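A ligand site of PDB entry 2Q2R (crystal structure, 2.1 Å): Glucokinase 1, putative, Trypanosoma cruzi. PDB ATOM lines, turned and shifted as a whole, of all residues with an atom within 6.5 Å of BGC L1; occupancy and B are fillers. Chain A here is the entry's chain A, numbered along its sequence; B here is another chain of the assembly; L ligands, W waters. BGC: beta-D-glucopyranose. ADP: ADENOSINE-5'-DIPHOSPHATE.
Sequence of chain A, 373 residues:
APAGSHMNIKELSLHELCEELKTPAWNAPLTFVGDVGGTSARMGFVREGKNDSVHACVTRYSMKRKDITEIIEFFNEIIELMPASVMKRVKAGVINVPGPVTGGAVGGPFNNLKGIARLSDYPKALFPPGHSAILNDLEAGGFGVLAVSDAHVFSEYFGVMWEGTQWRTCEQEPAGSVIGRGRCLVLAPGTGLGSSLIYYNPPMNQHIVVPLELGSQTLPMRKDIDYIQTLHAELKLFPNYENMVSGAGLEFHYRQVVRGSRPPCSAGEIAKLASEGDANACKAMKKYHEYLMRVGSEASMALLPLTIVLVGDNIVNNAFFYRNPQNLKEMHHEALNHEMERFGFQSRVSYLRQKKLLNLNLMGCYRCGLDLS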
ATOM      1  N   VAL A  97      29.522 -28.960   7.533  1.00  0.00           N
ATOM      2  CA  VAL A  97      30.328 -28.168   8.462  1.00  0.00           C
ATOM      3  C   VAL A  97      29.505 -27.689   9.667  1.00  0.00           C
ATOM      4  O   VAL A  97      28.298 -27.472   9.576  1.00  0.00           O
ATOM      5  CB  VAL A  97      30.906 -26.926   7.765  1.00  0.00           C
ATOM      6  CG1 VAL A  97      31.888 -27.320   6.632  1.00  0.00           C
ATOM      7  CG2 VAL A  97      29.767 -26.064   7.226  1.00  0.00           C
ATOM      8  N   PRO A  98      30.154 -27.506  10.822  1.00  0.00           N
ATOM      9  CA  PRO A  98      29.380 -27.258  12.048  1.00  0.00           C
ATOM     10  C   PRO A  98      28.942 -25.806  12.213  1.00  0.00           C
ATOM     11  O   PRO A  98      29.145 -25.204  13.254  1.00  0.00           O
ATOM     12  CB  PRO A  98      30.364 -27.635  13.144  1.00  0.00           C
ATOM     13  CG  PRO A  98      31.695 -27.192  12.595  1.00  0.00           C
ATOM     14  CD  PRO A  98      31.608 -27.542  11.082  1.00  0.00           C
ATOM     15  N   GLY A  99      28.349 -25.231  11.181  1.00  0.00           N
ATOM     16  CA  GLY A  99      27.865 -23.847  11.290  1.00  0.00           C
ATOM     17  C   GLY A  99      26.794 -23.539  10.260  1.00  0.00           C
ATOM     18  O   GLY A  99      26.492 -24.368   9.411  1.00  0.00           O
ATOM     19  N   PRO A 100      26.214 -22.339  10.340  1.00  0.00           N
ATOM     20  CA  PRO A 100      25.146 -21.973   9.406  1.00  0.00           C
ATOM     21  C   PRO A 100      25.679 -21.847   7.981  1.00  0.00           C
ATOM     22  O   PRO A 100      26.693 -21.197   7.755  1.00  0.00           O
ATOM     23  CB  PRO A 100      24.687 -20.591   9.890  1.00  0.00           C
ATOM     24  CG  PRO A 100      25.322 -20.366  11.202  1.00  0.00           C
ATOM     25  CD  PRO A 100      26.500 -21.274  11.304  1.00  0.00           C
ATOM     26  N   PRO A 109      29.838 -17.760  10.267  1.00  0.00           N
ATOM     27  CA  PRO A 109      30.968 -18.134  11.124  1.00  0.00           C
ATOM     28  C   PRO A 109      30.698 -19.280  12.103  1.00  0.00           C
ATOM     29  O   PRO A 109      29.541 -19.576  12.420  1.00  0.00           O
ATOM     30  CB  PRO A 109      31.296 -16.834  11.876  1.00  0.00           C
ATOM     31  CG  PRO A 109      30.097 -15.981  11.764  1.00  0.00           C
ATOM     32  CD  PRO A 109      29.312 -16.409  10.565  1.00  0.00           C
ATOM     33  N   PHE A 110      31.777 -19.894  12.584  1.00  0.00           N
ATOM     34  CA  PHE A 110      31.693 -21.024  13.510  1.00  0.00           C
ATOM     35  C   PHE A 110      32.066 -20.586  14.933  1.00  0.00           C
ATOM     36  O   PHE A 110      32.902 -19.698  15.092  1.00  0.00           O
ATOM     37  CB  PHE A 110      32.608 -22.135  13.024  1.00  0.00           C
ATOM     38  CG  PHE A 110      32.407 -22.486  11.574  1.00  0.00           C
ATOM     39  CD1 PHE A 110      33.063 -21.779  10.582  1.00  0.00           C
ATOM     40  CD2 PHE A 110      31.546 -23.501  11.208  1.00  0.00           C
ATOM     41  CE1 PHE A 110      32.869 -22.078   9.240  1.00  0.00           C
ATOM     42  CE2 PHE A 110      31.335 -23.810   9.883  1.00  0.00           C
ATOM     43  CZ  PHE A 110      32.011 -23.098   8.887  1.00  0.00           C
ATOM     44  N   ASN A 111      31.460 -21.183  15.943  1.00  0.00           N
ATOM     45  CA  ASN A 111      31.806 -20.904  17.345  1.00  0.00           C
ATOM     46  C   ASN A 111      33.255 -21.260  17.674  1.00  0.00           C
ATOM     47  O   ASN A 111      33.954 -20.499  18.366  1.00  0.00           O
ATOM     48  CB  ASN A 111      30.852 -21.616  18.299  1.00  0.00           C
ATOM     49  CG  ASN A 111      29.608 -20.778  18.616  1.00  0.00           C
ATOM     50  OD1 ASN A 111      29.642 -19.922  19.520  1.00  0.00           O
ATOM     51  ND2 ASN A 111      28.503 -21.014  17.884  1.00  0.00           N
ATOM     52  N   ASN A 112      33.703 -22.405  17.153  1.00  0.00           N
ATOM     53  CA  ASN A 112      35.013 -22.958  17.484  1.00  0.00           C
ATOM     54  C   ASN A 112      35.942 -23.252  16.306  1.00  0.00           C
ATOM     55  O   ASN A 112      36.869 -24.068  16.415  1.00  0.00           O
ATOM     56  CB  ASN A 112      34.829 -24.218  18.317  1.00  0.00           C
ATOM     57  CG  ASN A 112      33.770 -25.142  17.728  1.00  0.00           C
ATOM     58  OD1 ASN A 112      32.965 -25.719  18.468  1.00  0.00           O
ATOM     59  ND2 ASN A 112      33.757 -25.285  16.388  1.00  0.00           N
ATOM     60  N   ASN A 136      25.066 -27.787   6.255  1.00  0.00           N
ATOM     61  CA  ASN A 136      25.304 -27.639   7.694  1.00  0.00           C
ATOM     62  C   ASN A 136      25.270 -29.079   8.240  1.00  0.00           C
ATOM     63  O   ASN A 136      24.696 -29.968   7.609  1.00  0.00           O
ATOM     64  CB  ASN A 136      24.217 -26.770   8.298  1.00  0.00           C
ATOM     65  CG  ASN A 136      24.135 -26.882   9.810  1.00  0.00           C
ATOM     66  OD1 ASN A 136      24.905 -26.266  10.530  1.00  0.00           O
ATOM     67  ND2 ASN A 136      23.212 -27.678  10.289  1.00  0.00           N
ATOM     68  N   ASP A 137      25.897 -29.325   9.390  1.00  0.00           N
ATOM     69  CA  ASP A 137      25.996 -30.690   9.908  1.00  0.00           C
ATOM     70  C   ASP A 137      24.651 -31.378  10.154  1.00  0.00           C
ATOM     71  O   ASP A 137      24.449 -32.490   9.664  1.00  0.00           O
ATOM     72  CB  ASP A 137      26.968 -30.831  11.085  1.00  0.00           C
ATOM     73  CG  ASP A 137      26.703 -29.860  12.227  1.00  0.00           C
ATOM     74  OD1 ASP A 137      25.846 -28.969  12.084  1.00  0.00           O
ATOM     75  OD2 ASP A 137      27.372 -29.989  13.297  1.00  0.00           O
ATOM     76  N   LEU A 138      23.738 -30.719  10.857  1.00  0.00           N
ATOM     77  CA  LEU A 138      22.394 -31.265  11.070  1.00  0.00           C
ATOM     78  C   LEU A 138      21.514 -31.277   9.847  1.00  0.00           C
ATOM     79  O   LEU A 138      20.502 -31.979   9.835  1.00  0.00           O
ATOM     80  CB  LEU A 138      21.651 -30.564  12.205  1.00  0.00           C
ATOM     81  CG  LEU A 138      21.952 -31.213  13.558  1.00  0.00           C
ATOM     82  CD1 LEU A 138      21.298 -32.596  13.682  1.00  0.00           C
ATOM     83  CD2 LEU A 138      23.464 -31.364  13.696  1.00  0.00           C
ATOM     84  N   ALA A 188      21.027 -32.781  17.827  1.00  0.00           N
ATOM     85  CA  ALA A 188      22.292 -33.465  18.137  1.00  0.00           C
ATOM     86  C   ALA A 188      23.110 -32.689  19.168  1.00  0.00           C
ATOM     87  O   ALA A 188      23.714 -31.689  18.820  1.00  0.00           O
ATOM     88  CB  ALA A 188      23.106 -33.626  16.842  1.00  0.00           C
ATOM     89  N   GLY A 190      26.421 -32.243  21.217  1.00  0.00           N
ATOM     90  CA  GLY A 190      27.808 -32.652  21.357  1.00  0.00           C
ATOM     91  C   GLY A 190      28.670 -31.506  21.844  1.00  0.00           C
ATOM     92  O   GLY A 190      28.443 -30.978  22.950  1.00  0.00           O
ATOM     93  N   THR A 191      29.640 -31.103  21.029  1.00  0.00           N
ATOM     94  CA  THR A 191      30.430 -29.919  21.282  1.00  0.00           C
ATOM     95  C   THR A 191      29.519 -28.704  21.223  1.00  0.00           C
ATOM     96  O   THR A 191      29.556 -27.835  22.100  1.00  0.00           O
ATOM     97  CB  THR A 191      31.540 -29.746  20.232  1.00  0.00           C
ATOM     98  OG1 THR A 191      32.504 -30.790  20.415  1.00  0.00           O
ATOM     99  CG2 THR A 191      32.237 -28.384  20.381  1.00  0.00           C
ATOM    100  N   GLY A 192      28.688 -28.656  20.187  1.00  0.00           N
ATOM    101  CA  GLY A 192      27.589 -27.696  20.134  1.00  0.00           C
ATOM    102  C   GLY A 192      26.247 -28.409  20.186  1.00  0.00           C
ATOM    103  O   GLY A 192      26.172 -29.611  20.353  1.00  0.00           O
ATOM    104  N   LEU A 193      25.172 -27.669  20.022  1.00  0.00           N
ATOM    105  CA  LEU A 193      23.853 -28.285  19.926  1.00  0.00           C
ATOM    106  C   LEU A 193      23.296 -28.025  18.540  1.00  0.00           C
ATOM    107  O   LEU A 193      22.930 -26.904  18.246  1.00  0.00           O
ATOM    108  CB  LEU A 193      22.934 -27.713  21.007  1.00  0.00           C
ATOM    109  CG  LEU A 193      21.444 -28.067  20.954  1.00  0.00           C
ATOM    110  CD1 LEU A 193      21.228 -29.585  21.008  1.00  0.00           C
ATOM    111  CD2 LEU A 193      20.736 -27.354  22.125  1.00  0.00           C
ATOM    112  N   GLY A 194      23.250 -29.052  17.692  1.00  0.00           N
ATOM    113  CA  GLY A 194      22.645 -28.940  16.366  1.00  0.00           C
ATOM    114  C   GLY A 194      21.139 -29.173  16.386  1.00  0.00           C
ATOM    115  O   GLY A 194      20.610 -29.813  17.300  1.00  0.00           O
ATOM    116  N   SER A 195      20.457 -28.590  15.391  1.00  0.00           N
ATOM    117  CA  SER A 195      19.010 -28.729  15.220  1.00  0.00           C
ATOM    118  C   SER A 195      18.646 -28.551  13.752  1.00  0.00           C
ATOM    119  O   SER A 195      19.159 -27.652  13.106  1.00  0.00           O
ATOM    120  CB  SER A 195      18.313 -27.629  15.982  1.00  0.00           C
ATOM    121  OG  SER A 195      18.876 -26.399  15.602  1.00  0.00           O
ATOM    122  N   LEU A 212      18.406 -25.189  11.156  1.00  0.00           N
ATOM    123  CA  LEU A 212      18.029 -24.228  12.181  1.00  0.00           C
ATOM    124  C   LEU A 212      19.187 -24.004  13.139  1.00  0.00           C
ATOM    125  O   LEU A 212      20.160 -24.749  13.131  1.00  0.00           O
ATOM    126  CB  LEU A 212      16.827 -24.736  12.960  1.00  0.00           C
ATOM    127  CG  LEU A 212      15.544 -25.111  12.210  1.00  0.00           C
ATOM    128  CD1 LEU A 212      14.697 -25.974  13.085  1.00  0.00           C
ATOM    129  CD2 LEU A 212      14.803 -23.882  11.830  1.00  0.00           C
ATOM    130  N   GLU A 213      19.057 -22.988  13.984  1.00  0.00           N
ATOM    131  CA  GLU A 213      20.081 -22.706  14.973  1.00  0.00           C
ATOM    132  C   GLU A 213      19.416 -22.442  16.302  1.00  0.00           C
ATOM    133  O   GLU A 213      19.596 -21.374  16.843  1.00  0.00           O
ATOM    134  CB  GLU A 213      20.852 -21.441  14.573  1.00  0.00           C
ATOM    135  CG  GLU A 213      21.746 -21.542  13.346  1.00  0.00           C
ATOM    136  CD  GLU A 213      22.929 -22.450  13.533  1.00  0.00           C
ATOM    137  OE1 GLU A 213      23.481 -22.481  14.671  1.00  0.00           O
ATOM    138  OE2 GLU A 213      23.323 -23.146  12.555  1.00  0.00           O
ATOM    139  N   SER A 216      21.529 -21.452  19.594  1.00  0.00           N
ATOM    140  CA  SER A 216      22.025 -20.115  19.813  1.00  0.00           C
ATOM    141  C   SER A 216      20.999 -19.077  20.282  1.00  0.00           C
ATOM    142  O   SER A 216      21.358 -17.908  20.490  1.00  0.00           O
ATOM    143  CB  SER A 216      22.754 -19.632  18.567  1.00  0.00           C
ATOM    144  OG  SER A 216      23.881 -20.469  18.356  1.00  0.00           O
ATOM    145  N   GLU A 242      22.662 -23.838  23.987  1.00  0.00           N
ATOM    146  CA  GLU A 242      23.888 -24.588  23.809  1.00  0.00           C
ATOM    147  C   GLU A 242      24.789 -24.450  25.025  1.00  0.00           C
ATOM    148  O   GLU A 242      25.457 -25.410  25.415  1.00  0.00           O
ATOM    149  CB  GLU A 242      24.651 -24.096  22.590  1.00  0.00           C
ATOM    150  CG  GLU A 242      25.815 -24.947  22.155  1.00  0.00           C
ATOM    151  CD  GLU A 242      26.336 -24.493  20.820  1.00  0.00           C
ATOM    152  OE1 GLU A 242      26.052 -25.154  19.776  1.00  0.00           O
ATOM    153  OE2 GLU A 242      27.029 -23.467  20.777  1.00  0.00           O
ATOM    154  N   MET B 301      18.322 -15.392  14.603  1.00  0.00           N
ATOM    155  CA  MET B 301      19.282 -16.418  14.962  1.00  0.00           C
ATOM    156  C   MET B 301      18.741 -17.790  14.621  1.00  0.00           C
ATOM    157  O   MET B 301      19.323 -18.486  13.820  1.00  0.00           O
ATOM    158  CB  MET B 301      19.648 -16.381  16.443  1.00  0.00           C
ATOM    159  CG  MET B 301      20.877 -17.293  16.768  1.00  0.00           C
ATOM    160  SD  MET B 301      22.445 -16.773  15.955  1.00  0.00           S
ATOM    161  CE  MET B 301      22.580 -17.977  14.645  1.00  0.00           C
ATOM    162  N   PHE B 345      24.936 -12.089  13.142  1.00  0.00           N
ATOM    163  CA  PHE B 345      23.742 -12.800  12.675  1.00  0.00           C
ATOM    164  C   PHE B 345      22.498 -11.950  12.590  1.00  0.00           C
ATOM    165  O   PHE B 345      21.671 -12.118  11.691  1.00  0.00           O
ATOM    166  CB  PHE B 345      23.477 -14.081  13.491  1.00  0.00           C
ATOM    167  CG  PHE B 345      24.456 -15.176  13.209  1.00  0.00           C
ATOM    168  CD1 PHE B 345      24.417 -15.862  11.982  1.00  0.00           C
ATOM    169  CD2 PHE B 345      25.441 -15.517  14.129  1.00  0.00           C
ATOM    170  CE1 PHE B 345      25.352 -16.857  11.708  1.00  0.00           C
ATOM    171  CE2 PHE B 345      26.352 -16.541  13.857  1.00  0.00           C
ATOM    172  CZ  PHE B 345      26.306 -17.195  12.630  1.00  0.00           C
HETATM  173  C2  BGC L   1      26.469 -24.434  15.306  1.00  0.00           C
HETATM  174  C3  BGC L   1      25.487 -25.241  14.483  1.00  0.00           C
HETATM  175  C4  BGC L   1      25.814 -26.710  14.548  1.00  0.00           C
HETATM  176  C5  BGC L   1      25.894 -27.144  16.009  1.00  0.00           C
HETATM  177  C6  BGC L   1      26.250 -28.649  16.011  1.00  0.00           C
HETATM  178  C1  BGC L   1      26.375 -24.940  16.744  1.00  0.00           C
HETATM  179  O1  BGC L   1      27.041 -24.102  17.710  1.00  0.00           O
HETATM  180  O2  BGC L   1      26.055 -23.061  15.263  1.00  0.00           O
HETATM  181  O3  BGC L   1      25.441 -24.793  13.121  1.00  0.00           O
HETATM  182  O4  BGC L   1      24.724 -27.400  13.926  1.00  0.00           O
HETATM  183  O5  BGC L   1      26.781 -26.315  16.853  1.00  0.00           O
HETATM  184  O6  BGC L   1      27.587 -28.818  15.601  1.00  0.00           O
HETATM  185  PB  ADP L   2      31.452 -32.696  17.796  1.00  0.00           P
HETATM  186  O1B ADP L   2      32.756 -32.117  18.294  1.00  0.00           O
HETATM  187  O2B ADP L   2      30.232 -32.109  18.498  1.00  0.00           O
HETATM  188  O3B ADP L   2      31.375 -32.743  16.284  1.00  0.00           O
HETATM  189  PA  ADP L   2      30.495 -35.140  19.009  1.00  0.00           P
HETATM  190  O1A ADP L   2      31.048 -36.549  18.958  1.00  0.00           O
HETATM  191  O2A ADP L   2      29.120 -34.841  18.491  1.00  0.00           O
HETATM  192  O3A ADP L   2      31.561 -34.259  18.153  1.00  0.00           O
HETATM  193  O5' ADP L   2      30.644 -34.619  20.516  1.00  0.00           O
HETATM  194  C5' ADP L   2      31.927 -34.604  21.125  1.00  0.00           C
HETATM  195  C4' ADP L   2      31.893 -33.622  22.286  1.00  0.00           C
HETATM  196  O4' ADP L   2      30.766 -33.873  23.131  1.00  0.00           O
HETATM  197  C3' ADP L   2      33.123 -33.789  23.173  1.00  0.00           C
HETATM  198  O3' ADP L   2      34.199 -32.935  22.756  1.00  0.00           O
HETATM  199  C2' ADP L   2      32.612 -33.464  24.573  1.00  0.00           C
HETATM  200  O2' ADP L   2      32.713 -32.052  24.785  1.00  0.00           O
HETATM  201  C1' ADP L   2      31.141 -33.859  24.513  1.00  0.00           C
HETATM  202  N9  ADP L   2      30.919 -35.254  25.004  1.00  0.00           N
HETATM  203  C8  ADP L   2      31.789 -36.289  24.954  1.00  0.00           C
HETATM  204  N7  ADP L   2      31.236 -37.423  25.469  1.00  0.00           N
HETATM  205  C5  ADP L   2      29.990 -37.121  25.864  1.00  0.00           C
HETATM  206  C6  ADP L   2      28.852 -37.831  26.488  1.00  0.00           C
HETATM  207  N6  ADP L   2      28.949 -39.157  26.808  1.00  0.00           N
HETATM  208  N1  ADP L   2      27.711 -37.134  26.722  1.00  0.00           N
HETATM  209  C2  ADP L   2      27.591 -35.833  26.414  1.00  0.00           C
HETATM  210  N3  ADP L   2      28.580 -35.116  25.842  1.00  0.00           N
HETATM  211  C4  ADP L   2      29.777 -35.693  25.557  1.00  0.00           C
HETATM  212  O   HOH W   1      28.289 -21.691  15.078  1.00  0.00           O
HETATM  213  O   HOH W   2      28.649 -30.363  17.967  1.00  0.00           O
HETATM  214  O   HOH W   3      22.039 -26.507  14.083  1.00  0.00           O
HETATM  215  O   HOH W   4      29.721 -26.334  17.339  1.00  0.00           O
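Merely in contact with BGC L1: Gly 99 (3.2 Å), Pro 98 (3.5 Å), Gly 194 (3.5 Å), Gly 192 (3.7 Å), Leu 193 (3.7 Å) and Pro 100 (3.8 Å).
Hydrophobic or aromatic side chains that line BGC L1: Pro 98.
11 residues have an atom within 4 Å of BGC L1: Pro 98, Gly 99, Pro 100, Asn 111, Asn 136, Asp 137, Gly 192, Leu 193, Gly 194, Glu 213 and Glu 242.
The nearest printed residue that does not touch BGC L1 is Leu 138 (4.2 Å).
OE1 of Glu 242 sits at hydrogen-bond distance from N of Leu 193, 2.7 Å away.
The side-chain amide oxygen of Asn 136 sits close to the side-chain carboxylate of Asp 137, 3.3 Å away.
O of Val 97 is in hydrogen-bond range of N of Asp 137, 3.0 Å away.
The side-chain amide oxygen (OD1) of Asn 136 sits close to the backbone carbonyl oxygen (O) of Gly 99, 2.7 Å away.
The side-chain amide nitrogen of Asn 136 sits close to the backbone NH of Leu 138 (3.1 Å).
The backbone NH (N) of Gly 194 lies within hydrogen-bond range of the backbone carbonyl oxygen (O) of Ala 188 (2.9 Å).
Water W1 bridges O2 of BGC L1 (2.6 Å) and ND2 of Asn 111 (2.9 Å).
Water W3 lies within hydrogen-bond range of the backbone carbonyl oxygen (O) of Leu 212, an oxygen (O4) of BGC L1 and the backbone NH (N) of Ser 195.
Water W4 lies within hydrogen-bond range of O5 of BGC L1 and OD1 of Asn 112.
Water W2 lies within hydrogen-bond range of O2B of ADP L2, N of Gly 192, O6 of BGC L1 and N of Thr 191.
An oxygen (O1) of BGC L1 lies within hydrogen-bond range of the side-chain carboxylate (OE1) of Glu 242, 2.5 Å away.
The side-chain carboxylate (OD2) of Asp 137 is in hydrogen-bond range of an oxygen (O6) of BGC L1 (2.6 Å).
An oxygen (O2) of BGC L1 sits at hydrogen-bond distance from the side-chain carboxylate (OE1) of Glu 213 (2.7 Å).
An oxygen (O3) of BGC L1 is in hydrogen-bond range of the side-chain amide oxygen (OD1) of Asn 136 (3.0 Å).
O1 of BGC L1 sits at hydrogen-bond distance from ND2 of Asn 111 (3.4 Å).
The backbone NH of Thr 191 lies within hydrogen-bond range of an oxygen (O2B) of ADP L2.
O1B of ADP L2 is in hydrogen-bond range of OG1 of Thr 191, 2.5 Å away.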
